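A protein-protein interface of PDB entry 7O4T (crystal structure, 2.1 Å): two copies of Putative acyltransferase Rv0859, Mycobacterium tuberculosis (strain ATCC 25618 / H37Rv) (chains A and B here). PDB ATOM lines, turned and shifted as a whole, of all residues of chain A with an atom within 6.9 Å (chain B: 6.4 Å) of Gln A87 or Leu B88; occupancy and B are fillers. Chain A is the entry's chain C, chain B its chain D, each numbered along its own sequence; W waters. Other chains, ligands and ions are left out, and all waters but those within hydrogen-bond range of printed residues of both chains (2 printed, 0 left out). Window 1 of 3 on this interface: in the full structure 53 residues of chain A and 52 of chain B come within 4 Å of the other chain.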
ATOM      1  N   VAL A  54     -10.595 -13.925  -3.293  1.00  0.00           N
ATOM      2  CA  VAL A  54     -10.865 -13.607  -1.895  1.00  0.00           C
ATOM      3  C   VAL A  54     -10.112 -12.326  -1.571  1.00  0.00           C
ATOM      4  O   VAL A  54      -8.879 -12.285  -1.663  1.00  0.00           O
ATOM      5  CB  VAL A  54     -10.451 -14.747  -0.952  1.00  0.00           C
ATOM      6  CG1 VAL A  54     -10.603 -14.318   0.497  1.00  0.00           C
ATOM      7  CG2 VAL A  54     -11.281 -15.989  -1.226  1.00  0.00           C
ATOM      8  N   ILE A  55     -10.848 -11.279  -1.212  1.00  0.00           N
ATOM      9  CA  ILE A  55     -10.285  -9.948  -1.012  1.00  0.00           C
ATOM     10  C   ILE A  55     -10.492  -9.564   0.445  1.00  0.00           C
ATOM     11  O   ILE A  55     -11.634  -9.416   0.897  1.00  0.00           O
ATOM     12  CB  ILE A  55     -10.925  -8.917  -1.953  1.00  0.00           C
ATOM     13  CG1 ILE A  55     -10.825  -9.394  -3.406  1.00  0.00           C
ATOM     14  CG2 ILE A  55     -10.260  -7.559  -1.795  1.00  0.00           C
ATOM     15  CD1 ILE A  55     -11.498  -8.474  -4.397  1.00  0.00           C
ATOM     16  N   LEU A  56      -9.396  -9.398   1.177  1.00  0.00           N
ATOM     17  CA  LEU A  56      -9.445  -9.097   2.602  1.00  0.00           C
ATOM     18  C   LEU A  56      -8.733  -7.783   2.883  1.00  0.00           C
ATOM     19  O   LEU A  56      -7.589  -7.587   2.457  1.00  0.00           O
ATOM     20  CB  LEU A  56      -8.806 -10.218   3.426  1.00  0.00           C
ATOM     21  CG  LEU A  56      -9.489 -11.586   3.438  1.00  0.00           C
ATOM     22  CD1 LEU A  56      -8.777 -12.518   4.417  1.00  0.00           C
ATOM     23  CD2 LEU A  56     -10.959 -11.448   3.795  1.00  0.00           C
ATOM     24  N   GLY A  57      -9.406  -6.892   3.607  1.00  0.00           N
ATOM     25  CA  GLY A  57      -8.747  -5.705   4.121  1.00  0.00           C
ATOM     26  C   GLY A  57      -7.971  -6.022   5.392  1.00  0.00           C
ATOM     27  O   GLY A  57      -8.374  -6.857   6.202  1.00  0.00           O
ATOM     28  N   CYS A  58      -6.833  -5.350   5.550  1.00  0.00           N
ATOM     29  CA  CYS A  58      -5.984  -5.535   6.727  1.00  0.00           C
ATOM     30  C   CYS A  58      -5.066  -4.329   6.825  1.00  0.00           C
ATOM     31  O   CYS A  58      -4.263  -4.088   5.917  1.00  0.00           O
ATOM     32  CB  CYS A  58      -5.177  -6.833   6.633  1.00  0.00           C
ATOM     33  SG  CYS A  58      -4.302  -7.284   8.163  1.00  0.00           S
ATOM     34  N   VAL A  59      -5.182  -3.574   7.918  1.00  0.00           N
ATOM     35  CA  VAL A  59      -4.446  -2.321   8.030  1.00  0.00           C
ATOM     36  C   VAL A  59      -3.012  -2.556   8.497  1.00  0.00           C
ATOM     37  O   VAL A  59      -2.111  -1.778   8.162  1.00  0.00           O
ATOM     38  CB  VAL A  59      -5.200  -1.354   8.958  1.00  0.00           C
ATOM     39  CG1 VAL A  59      -4.444  -0.038   9.113  1.00  0.00           C
ATOM     40  CG2 VAL A  59      -6.595  -1.096   8.408  1.00  0.00           C
ATOM     41  N   SER A  60      -2.764  -3.629   9.247  1.00  0.00           N
ATOM     42  CA  SER A  60      -1.429  -3.958   9.745  1.00  0.00           C
ATOM     43  C   SER A  60      -1.024  -5.336   9.228  1.00  0.00           C
ATOM     44  O   SER A  60      -1.016  -6.319   9.981  1.00  0.00           O
ATOM     45  CB  SER A  60      -1.387  -3.910  11.271  1.00  0.00           C
ATOM     46  OG  SER A  60      -1.761  -2.627  11.747  1.00  0.00           O
ATOM     47  N   PRO A  61      -0.674  -5.441   7.942  1.00  0.00           N
ATOM     48  CA  PRO A  61      -0.346  -6.755   7.353  1.00  0.00           C
ATOM     49  C   PRO A  61       1.077  -7.199   7.672  1.00  0.00           C
ATOM     50  O   PRO A  61       1.944  -7.332   6.802  1.00  0.00           O
ATOM     51  CB  PRO A  61      -0.568  -6.504   5.858  1.00  0.00           C
ATOM     52  CG  PRO A  61      -0.191  -5.071   5.677  1.00  0.00           C
ATOM     53  CD  PRO A  61      -0.591  -4.356   6.948  1.00  0.00           C
ATOM     54  N   GLN A  65      -0.491 -11.378  10.435  1.00  0.00           N
ATOM     55  CA  GLN A  65      -1.332 -10.849   9.370  1.00  0.00           C
ATOM     56  C   GLN A  65      -0.542 -10.522   8.109  1.00  0.00           C
ATOM     57  O   GLN A  65      -1.077  -9.878   7.203  1.00  0.00           O
ATOM     58  CB  GLN A  65      -2.092  -9.615   9.870  1.00  0.00           C
ATOM     59  CG  GLN A  65      -2.970  -9.918  11.075  1.00  0.00           C
ATOM     60  CD  GLN A  65      -3.790  -8.730  11.552  1.00  0.00           C
ATOM     61  OE1 GLN A  65      -4.851  -8.904  12.149  1.00  0.00           O
ATOM     62  NE2 GLN A  65      -3.295  -7.521  11.309  1.00  0.00           N
ATOM     63  N   GLY A  67       2.130 -11.707   4.733  1.00  0.00           N
ATOM     64  CA  GLY A  67       2.201 -12.742   3.711  1.00  0.00           C
ATOM     65  C   GLY A  67       0.891 -13.036   3.014  1.00  0.00           C
ATOM     66  O   GLY A  67       0.573 -14.209   2.775  1.00  0.00           O
ATOM     67  N   ASP A  68       0.127 -11.995   2.673  1.00  0.00           N
ATOM     68  CA  ASP A  68      -1.159 -12.141   1.997  1.00  0.00           C
ATOM     69  C   ASP A  68      -2.075 -13.077   2.775  1.00  0.00           C
ATOM     70  O   ASP A  68      -2.261 -14.235   2.389  1.00  0.00           O
ATOM     71  CB  ASP A  68      -0.957 -12.649   0.564  1.00  0.00           C
ATOM     72  CG  ASP A  68      -2.223 -12.569  -0.274  1.00  0.00           C
ATOM     73  OD1 ASP A  68      -3.273 -12.136   0.249  1.00  0.00           O
ATOM     74  OD2 ASP A  68      -2.166 -12.940  -1.467  1.00  0.00           O
ATOM     75  N   ILE A  69      -2.654 -12.580   3.871  1.00  0.00           N
ATOM     76  CA  ILE A  69      -3.477 -13.421   4.732  1.00  0.00           C
ATOM     77  C   ILE A  69      -4.697 -13.958   3.994  1.00  0.00           C
ATOM     78  O   ILE A  69      -5.243 -14.998   4.377  1.00  0.00           O
ATOM     79  CB  ILE A  69      -3.880 -12.639   6.002  1.00  0.00           C
ATOM     80  CG1 ILE A  69      -4.449 -13.588   7.061  1.00  0.00           C
ATOM     81  CG2 ILE A  69      -4.873 -11.529   5.666  1.00  0.00           C
ATOM     82  CD1 ILE A  69      -4.733 -12.921   8.390  1.00  0.00           C
ATOM     83  N   ALA A  70      -5.129 -13.285   2.923  1.00  0.00           N
ATOM     84  CA  ALA A  70      -6.247 -13.795   2.136  1.00  0.00           C
ATOM     85  C   ALA A  70      -5.883 -15.097   1.433  1.00  0.00           C
ATOM     86  O   ALA A  70      -6.667 -16.053   1.439  1.00  0.00           O
ATOM     87  CB  ALA A  70      -6.700 -12.743   1.124  1.00  0.00           C
ATOM     88  N   ARG A  71      -4.697 -15.154   0.821  1.00  0.00           N
ATOM     89  CA  ARG A  71      -4.254 -16.398   0.200  1.00  0.00           C
ATOM     90  C   ARG A  71      -4.031 -17.479   1.249  1.00  0.00           C
ATOM     91  O   ARG A  71      -4.339 -18.655   1.015  1.00  0.00           O
ATOM     92  CB  ARG A  71      -2.978 -16.163  -0.609  1.00  0.00           C
ATOM     93  CG  ARG A  71      -2.474 -17.398  -1.338  1.00  0.00           C
ATOM     94  CD  ARG A  71      -3.559 -17.973  -2.234  1.00  0.00           C
ATOM     95  NE  ARG A  71      -3.101 -19.114  -3.022  1.00  0.00           N
ATOM     96  CZ  ARG A  71      -3.865 -19.774  -3.889  1.00  0.00           C
ATOM     97  NH1 ARG A  71      -5.123 -19.402  -4.084  1.00  0.00           N
ATOM     98  NH2 ARG A  71      -3.373 -20.799  -4.567  1.00  0.00           N
ATOM     99  N   GLY A  85      -6.840 -14.781  -3.800  1.00  0.00           N
ATOM    100  CA  GLY A  85      -6.519 -14.294  -2.475  1.00  0.00           C
ATOM    101  C   GLY A  85      -5.600 -13.091  -2.521  1.00  0.00           C
ATOM    102  O   GLY A  85      -4.433 -13.212  -2.905  1.00  0.00           O
ATOM    103  N   VAL A  86      -6.110 -11.923  -2.140  1.00  0.00           N
ATOM    104  CA  VAL A  86      -5.349 -10.681  -2.192  1.00  0.00           C
ATOM    105  C   VAL A  86      -5.672  -9.855  -0.954  1.00  0.00           C
ATOM    106  O   VAL A  86      -6.829  -9.784  -0.524  1.00  0.00           O
ATOM    107  CB  VAL A  86      -5.643  -9.893  -3.491  1.00  0.00           C
ATOM    108  CG1 VAL A  86      -7.142  -9.727  -3.692  1.00  0.00           C
ATOM    109  CG2 VAL A  86      -4.944  -8.539  -3.480  1.00  0.00           C
ATOM    110  N   GLN A  87      -4.643  -9.249  -0.370  1.00  0.00           N
ATOM    111  CA  GLN A  87      -4.775  -8.366   0.779  1.00  0.00           C
ATOM    112  C   GLN A  87      -4.670  -6.919   0.319  1.00  0.00           C
ATOM    113  O   GLN A  87      -3.882  -6.602  -0.575  1.00  0.00           O
ATOM    114  CB  GLN A  87      -3.691  -8.674   1.821  1.00  0.00           C
ATOM    115  CG  GLN A  87      -3.577  -7.668   2.968  1.00  0.00           C
ATOM    116  CD  GLN A  87      -2.631  -6.520   2.653  1.00  0.00           C
ATOM    117  OE1 GLN A  87      -1.599  -6.712   2.011  1.00  0.00           O
ATOM    118  NE2 GLN A  87      -2.987  -5.319   3.097  1.00  0.00           N
ATOM    119  N   LEU A  88      -5.466  -6.038   0.927  1.00  0.00           N
ATOM    120  CA  LEU A  88      -5.379  -4.620   0.609  1.00  0.00           C
ATOM    121  C   LEU A  88      -5.481  -3.791   1.881  1.00  0.00           C
ATOM    122  O   LEU A  88      -6.036  -4.223   2.895  1.00  0.00           O
ATOM    123  CB  LEU A  88      -6.447  -4.190  -0.413  1.00  0.00           C
ATOM    124  CG  LEU A  88      -7.949  -4.296  -0.147  1.00  0.00           C
ATOM    125  CD1 LEU A  88      -8.458  -3.149   0.715  1.00  0.00           C
ATOM    126  CD2 LEU A  88      -8.690  -4.329  -1.475  1.00  0.00           C
ATOM    127  N   ASN A  89      -4.932  -2.582   1.807  1.00  0.00           N
ATOM    128  CA  ASN A  89      -4.915  -1.658   2.936  1.00  0.00           C
ATOM    129  C   ASN A  89      -5.288  -0.271   2.434  1.00  0.00           C
ATOM    130  O   ASN A  89      -4.510   0.360   1.713  1.00  0.00           O
ATOM    131  CB  ASN A  89      -3.546  -1.639   3.615  1.00  0.00           C
ATOM    132  CG  ASN A  89      -3.443  -0.582   4.699  1.00  0.00           C
ATOM    133  OD1 ASN A  89      -4.455  -0.106   5.220  1.00  0.00           O
ATOM    134  ND2 ASN A  89      -2.216  -0.211   5.047  1.00  0.00           N
ATOM    135  N   ARG A  90      -6.479   0.194   2.809  1.00  0.00           N
ATOM    136  CA  ARG A  90      -6.821   1.603   2.685  1.00  0.00           C
ATOM    137  C   ARG A  90      -7.247   2.116   4.056  1.00  0.00           C
ATOM    138  O   ARG A  90      -8.282   2.779   4.188  1.00  0.00           O
ATOM    139  CB  ARG A  90      -7.924   1.829   1.651  1.00  0.00           C
ATOM    140  CG  ARG A  90      -8.020   3.276   1.171  1.00  0.00           C
ATOM    141  CD  ARG A  90      -9.409   3.615   0.650  1.00  0.00           C
ATOM    142  NE  ARG A  90      -9.673   3.010  -0.650  1.00  0.00           N
ATOM    143  CZ  ARG A  90      -9.282   3.535  -1.806  1.00  0.00           C
ATOM    144  NH1 ARG A  90      -8.602   4.671  -1.819  1.00  0.00           N
ATOM    145  NH2 ARG A  90      -9.568   2.924  -2.948  1.00  0.00           N
ATOM    146  N   SER A  94     -10.688  -0.325   4.772  1.00  0.00           N
ATOM    147  CA  SER A  94     -10.197  -1.484   4.031  1.00  0.00           C
ATOM    148  C   SER A  94     -11.276  -2.548   3.873  1.00  0.00           C
ATOM    149  O   SER A  94     -11.397  -3.164   2.806  1.00  0.00           O
ATOM    150  CB  SER A  94      -8.967  -2.072   4.729  1.00  0.00           C
ATOM    151  OG  SER A  94      -7.942  -1.103   4.860  1.00  0.00           O
ATOM    152  N   ILE B  55      -3.407   2.968  -6.896  1.00  0.00           N
ATOM    153  CA  ILE B  55      -3.365   1.579  -6.454  1.00  0.00           C
ATOM    154  C   ILE B  55      -1.955   1.058  -6.694  1.00  0.00           C
ATOM    155  O   ILE B  55      -1.517   0.938  -7.845  1.00  0.00           O
ATOM    156  CB  ILE B  55      -4.403   0.723  -7.190  1.00  0.00           C
ATOM    157  CG1 ILE B  55      -5.779   1.391  -7.137  1.00  0.00           C
ATOM    158  CG2 ILE B  55      -4.464  -0.665  -6.592  1.00  0.00           C
ATOM    159  CD1 ILE B  55      -6.837   0.672  -7.945  1.00  0.00           C
ATOM    160  N   LEU B  56      -1.241   0.736  -5.617  1.00  0.00           N
ATOM    161  CA  LEU B  56       0.145   0.292  -5.702  1.00  0.00           C
ATOM    162  C   LEU B  56       0.284  -1.115  -5.141  1.00  0.00           C
ATOM    163  O   LEU B  56      -0.177  -1.397  -4.030  1.00  0.00           O
ATOM    164  CB  LEU B  56       1.081   1.242  -4.948  1.00  0.00           C
ATOM    165  CG  LEU B  56       1.255   2.648  -5.520  1.00  0.00           C
ATOM    166  CD1 LEU B  56       2.267   3.428  -4.699  1.00  0.00           C
ATOM    167  CD2 LEU B  56       1.677   2.587  -6.981  1.00  0.00           C
ATOM    168  N   GLY B  57       0.929  -1.991  -5.909  1.00  0.00           N
ATOM    169  CA  GLY B  57       1.267  -3.310  -5.405  1.00  0.00           C
ATOM    170  C   GLY B  57       2.546  -3.267  -4.581  1.00  0.00           C
ATOM    171  O   GLY B  57       3.480  -2.521  -4.877  1.00  0.00           O
ATOM    172  N   CYS B  58       2.574  -4.077  -3.526  1.00  0.00           N
ATOM    173  CA  CYS B  58       3.735  -4.146  -2.642  1.00  0.00           C
ATOM    174  C   CYS B  58       3.650  -5.447  -1.862  1.00  0.00           C
ATOM    175  O   CYS B  58       2.673  -5.667  -1.138  1.00  0.00           O
ATOM    176  CB  CYS B  58       3.779  -2.944  -1.698  1.00  0.00           C
ATOM    177  SG  CYS B  58       5.308  -2.796  -0.749  1.00  0.00           S
ATOM    178  N   VAL B  59       4.663  -6.299  -2.003  1.00  0.00           N
ATOM    179  CA  VAL B  59       4.620  -7.624  -1.394  1.00  0.00           C
ATOM    180  C   VAL B  59       5.121  -7.616   0.048  1.00  0.00           C
ATOM    181  O   VAL B  59       4.731  -8.477   0.846  1.00  0.00           O
ATOM    182  CB  VAL B  59       5.416  -8.618  -2.258  1.00  0.00           C
ATOM    183  CG1 VAL B  59       5.248 -10.043  -1.747  1.00  0.00           C
ATOM    184  CG2 VAL B  59       4.968  -8.518  -3.705  1.00  0.00           C
ATOM    185  N   PRO B  61       4.807  -4.875   2.611  1.00  0.00           N
ATOM    186  CA  PRO B  61       4.388  -3.537   3.085  1.00  0.00           C
ATOM    187  C   PRO B  61       4.706  -3.312   4.558  1.00  0.00           C
ATOM    188  O   PRO B  61       3.826  -3.219   5.422  1.00  0.00           O
ATOM    189  CB  PRO B  61       2.884  -3.545   2.797  1.00  0.00           C
ATOM    190  CG  PRO B  61       2.490  -4.966   2.954  1.00  0.00           C
ATOM    191  CD  PRO B  61       3.660  -5.791   2.472  1.00  0.00           C
ATOM    192  N   VAL B  86      -4.307   3.168  -2.167  1.00  0.00           N
ATOM    193  CA  VAL B  86      -4.498   1.862  -1.548  1.00  0.00           C
ATOM    194  C   VAL B  86      -3.348   0.945  -1.952  1.00  0.00           C
ATOM    195  O   VAL B  86      -2.928   0.927  -3.114  1.00  0.00           O
ATOM    196  CB  VAL B  86      -5.865   1.253  -1.932  1.00  0.00           C
ATOM    197  CG1 VAL B  86      -6.079   1.318  -3.434  1.00  0.00           C
ATOM    198  CG2 VAL B  86      -5.981  -0.182  -1.428  1.00  0.00           C
ATOM    199  N   GLN B  87      -2.823   0.203  -0.979  1.00  0.00           N
ATOM    200  CA  GLN B  87      -1.805  -0.813  -1.202  1.00  0.00           C
ATOM    201  C   GLN B  87      -2.468  -2.181  -1.285  1.00  0.00           C
ATOM    202  O   GLN B  87      -3.410  -2.466  -0.543  1.00  0.00           O
ATOM    203  CB  GLN B  87      -0.764  -0.790  -0.078  1.00  0.00           C
ATOM    204  CG  GLN B  87       0.200  -1.978  -0.054  1.00  0.00           C
ATOM    205  CD  GLN B  87      -0.297  -3.121   0.814  1.00  0.00           C
ATOM    206  OE1 GLN B  87      -0.819  -2.903   1.909  1.00  0.00           O
ATOM    207  NE2 GLN B  87      -0.144  -4.348   0.326  1.00  0.00           N
ATOM    208  N   LEU B  88      -1.983  -3.026  -2.195  1.00  0.00           N
ATOM    209  CA  LEU B  88      -2.464  -4.396  -2.288  1.00  0.00           C
ATOM    210  C   LEU B  88      -1.284  -5.349  -2.428  1.00  0.00           C
ATOM    211  O   LEU B  88      -0.179  -4.956  -2.812  1.00  0.00           O
ATOM    212  CB  LEU B  88      -3.461  -4.586  -3.449  1.00  0.00           C
ATOM    213  CG  LEU B  88      -3.076  -4.472  -4.926  1.00  0.00           C
ATOM    214  CD1 LEU B  88      -2.426  -5.749  -5.449  1.00  0.00           C
ATOM    215  CD2 LEU B  88      -4.315  -4.142  -5.746  1.00  0.00           C
ATOM    216  N   ASN B  89      -1.538  -6.616  -2.109  1.00  0.00           N
ATOM    217  CA  ASN B  89      -0.511  -7.653  -2.154  1.00  0.00           C
ATOM    218  C   ASN B  89      -1.139  -8.939  -2.671  1.00  0.00           C
ATOM    219  O   ASN B  89      -1.912  -9.585  -1.956  1.00  0.00           O
ATOM    220  CB  ASN B  89       0.116  -7.875  -0.774  1.00  0.00           C
ATOM    221  CG  ASN B  89       1.119  -9.021  -0.761  1.00  0.00           C
ATOM    222  OD1 ASN B  89       1.658  -9.406  -1.799  1.00  0.00           O
ATOM    223  ND2 ASN B  89       1.372  -9.570   0.422  1.00  0.00           N
ATOM    224  N   ARG B  90      -0.814  -9.303  -3.911  1.00  0.00           N
ATOM    225  CA  ARG B  90      -1.066 -10.652  -4.401  1.00  0.00           C
ATOM    226  C   ARG B  90       0.258 -11.262  -4.847  1.00  0.00           C
ATOM    227  O   ARG B  90       0.379 -11.758  -5.973  1.00  0.00           O
ATOM    228  CB  ARG B  90      -2.083 -10.656  -5.548  1.00  0.00           C
ATOM    229  CG  ARG B  90      -2.702 -12.030  -5.807  1.00  0.00           C
ATOM    230  CD  ARG B  90      -3.333 -12.128  -7.193  1.00  0.00           C
ATOM    231  NE  ARG B  90      -4.522 -11.291  -7.320  1.00  0.00           N
ATOM    232  CZ  ARG B  90      -5.760 -11.703  -7.064  1.00  0.00           C
ATOM    233  NH1 ARG B  90      -5.982 -12.947  -6.663  1.00  0.00           N
ATOM    234  NH2 ARG B  90      -6.780 -10.868  -7.208  1.00  0.00           N
ATOM    235  N   ALA B  93       2.309 -11.103  -8.595  1.00  0.00           N
ATOM    236  CA  ALA B  93       1.437 -10.440  -9.556  1.00  0.00           C
ATOM    237  C   ALA B  93       0.841  -9.143  -9.029  1.00  0.00           C
ATOM    238  O   ALA B  93      -0.070  -8.599  -9.663  1.00  0.00           O
ATOM    239  CB  ALA B  93       0.310 -11.377  -9.986  1.00  0.00           C
ATOM    240  N   SER B  94       1.337  -8.634  -7.897  1.00  0.00           N
ATOM    241  CA  SER B  94       0.754  -7.440  -7.291  1.00  0.00           C
ATOM    242  C   SER B  94       0.741  -6.267  -8.263  1.00  0.00           C
ATOM    243  O   SER B  94      -0.236  -5.511  -8.320  1.00  0.00           O
ATOM    244  CB  SER B  94       1.518  -7.071  -6.019  1.00  0.00           C
ATOM    245  OG  SER B  94       1.394  -8.080  -5.031  1.00  0.00           O
ATOM    246  N   GLY B  95       1.813  -6.102  -9.040  1.00  0.00           N
ATOM    247  CA  GLY B  95       1.874  -4.987  -9.972  1.00  0.00           C
ATOM    248  C   GLY B  95       0.841  -5.088 -11.078  1.00  0.00           C
ATOM    249  O   GLY B  95       0.225  -4.088 -11.457  1.00  0.00           O
ATOM    250  N   GLU B  97      -1.911  -6.980 -10.800  1.00  0.00           N
ATOM    251  CA  GLU B  97      -3.208  -6.954 -10.130  1.00  0.00           C
ATOM    252  C   GLU B  97      -3.670  -5.524  -9.889  1.00  0.00           C
ATOM    253  O   GLU B  97      -4.864  -5.221 -10.003  1.00  0.00           O
ATOM    254  CB  GLU B  97      -3.132  -7.728  -8.813  1.00  0.00           C
ATOM    255  CG  GLU B  97      -4.424  -7.716  -8.006  1.00  0.00           C
ATOM    256  CD  GLU B  97      -5.589  -8.333  -8.757  1.00  0.00           C
ATOM    257  OE1 GLU B  97      -5.374  -9.331  -9.480  1.00  0.00           O
ATOM    258  OE2 GLU B  97      -6.720  -7.816  -8.631  1.00  0.00           O
ATOM    259  N   ALA B  98      -2.739  -4.628  -9.555  1.00  0.00           N
ATOM    260  CA  ALA B  98      -3.093  -3.223  -9.396  1.00  0.00           C
ATOM    261  C   ALA B  98      -3.622  -2.639 -10.700  1.00  0.00           C
ATOM    262  O   ALA B  98      -4.630  -1.921 -10.706  1.00  0.00           O
ATOM    263  CB  ALA B  98      -1.884  -2.428  -8.905  1.00  0.00           C
ATOM    264  N   VAL B  99      -2.956  -2.942 -11.816  1.00  0.00           N
ATOM    265  CA  VAL B  99      -3.419  -2.466 -13.117  1.00  0.00           C
ATOM    266  C   VAL B  99      -4.783  -3.059 -13.441  1.00  0.00           C
ATOM    267  O   VAL B  99      -5.697  -2.355 -13.887  1.00  0.00           O
ATOM    268  CB  VAL B  99      -2.383  -2.801 -14.205  1.00  0.00           C
ATOM    269  CG1 VAL B  99      -2.981  -2.605 -15.592  1.00  0.00           C
ATOM    270  CG2 VAL B  99      -1.133  -1.952 -14.021  1.00  0.00           C
ATOM    271  N   THR B 101      -7.068  -4.224 -11.348  1.00  0.00           N
ATOM    272  CA  THR B 101      -8.076  -3.628 -10.476  1.00  0.00           C
ATOM    273  C   THR B 101      -8.438  -2.220 -10.932  1.00  0.00           C
ATOM    274  O   THR B 101      -9.616  -1.843 -10.936  1.00  0.00           O
ATOM    275  CB  THR B 101      -7.579  -3.617  -9.028  1.00  0.00           C
ATOM    276  OG1 THR B 101      -7.447  -4.965  -8.561  1.00  0.00           O
ATOM    277  CG2 THR B 101      -8.552  -2.868  -8.127  1.00  0.00           C
HETATM  278  O   HOH W   1      -0.034  -8.773   2.875  1.00  0.00           O
HETATM  279  O   HOH W   2       0.182  -1.260   3.607  1.00  0.00           O
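OE1 of Gln A87 lies within hydrogen-bond range of NE2 of Gln B87, 3.2 Å away.
N of Asn B89 sits at hydrogen-bond distance from O of Gln A87, at 2.8 Å.
The backbone NH (N) of Asn A89 sits at hydrogen-bond distance from the backbone carbonyl oxygen (O) of Gln B87.
The side-chain carboxylate (OD2) of Asp A68 sits close to the backbone carbonyl oxygen (O) of Asn B89 (3.4 Å).
The backbone NH of Leu A88 is in hydrogen-bond range of the backbone carbonyl oxygen of Leu A56, 3.0 Å away.
O of Val A59 lies within hydrogen-bond range of ND2 of Asn A89, 3.5 Å away.
The side-chain carboxylate (OD1) of Asp A68 lies close to the backbone NH (N) of Ala A70, at 3.5 Å.
OD1 of Asp A68 lies within hydrogen-bond range of N of Gln A87 (3.3 Å).
The backbone NH (N) of Leu B56 is in hydrogen-bond range of the backbone carbonyl oxygen (O) of Val B86.
The backbone carbonyl oxygen (O) of Leu B56 is in hydrogen-bond range of the backbone NH (N) of Leu B88, 3.0 Å away.
Of chain B, only Gln B87 (3.2 Å), Leu B88 (3.1 Å) and Asn B89 (2.8 Å) come within 4 Å of Gln A87.
Of chain A, only Gln A87 comes within 4 Å of Leu B88.
Of the printed residues of chain B, Leu A88 touches Gln B87.
Printed residues of chain B within 4 Å of Gly A85: Arg B90.
Of the printed residues of chain B, Asn A89 touches Val B86 (3.5 Å) and Gln B87 (2.8 Å).
Gly A57 touches none of the printed residues of chain B.
Printed residues of chain B that touch a printed residue of chain A: Pro B61, Val B86, Gln B87, Leu B88, Asn B89 and Arg B90.
Printed residues of chain A that touch a printed residue of chain B: Pro A61, Asp A68, Gly A85, Val A86, Gln A87, Leu A88, Asn A89 and Arg A90.
Among the printed residues, 13 pairs touch across the chains.
Among the printed residues, no Asp or Glu carboxylate lies within 4 Å of a Lys or Arg side-chain nitrogen of the other chain.
Pro B61 touches its own counterpart, Pro A61.
Val A86 touches Asn B89, and with the chains exchanged Asn A89 touches Val B86.
Gln A87 touches its own counterpart, Gln B87.
Gln A87 touches Asn B89, and with the chains exchanged Asn A89 touches Gln B87.
Of the 13 pairs that touch across the chains among the printed residues, 10 have their exchanged pair printed and touching as well.
Among the printed residues, merely in contact across the chains: Pro A61 with Pro B61, Asp A68 with Arg B90, Gly A85 with Arg B90, Val A86 with Asn B89, Val A86 with Arg B90, Gln A87 with Leu B88, Leu A88 with Gln B87, Asn A89 with Val B86 and Arg A90 with Val B86.
Water W2 bridges the side-chain amide oxygen of Gln B87 (2.6 Å) and the side-chain amide nitrogen of Asn A89 (3.0 Å).
Water W1 lies within hydrogen-bond range of OE1 of Gln A87 (2.7 Å), ND2 of Asn B89 (2.9 Å) and N of Asp A68 (3.2 Å).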
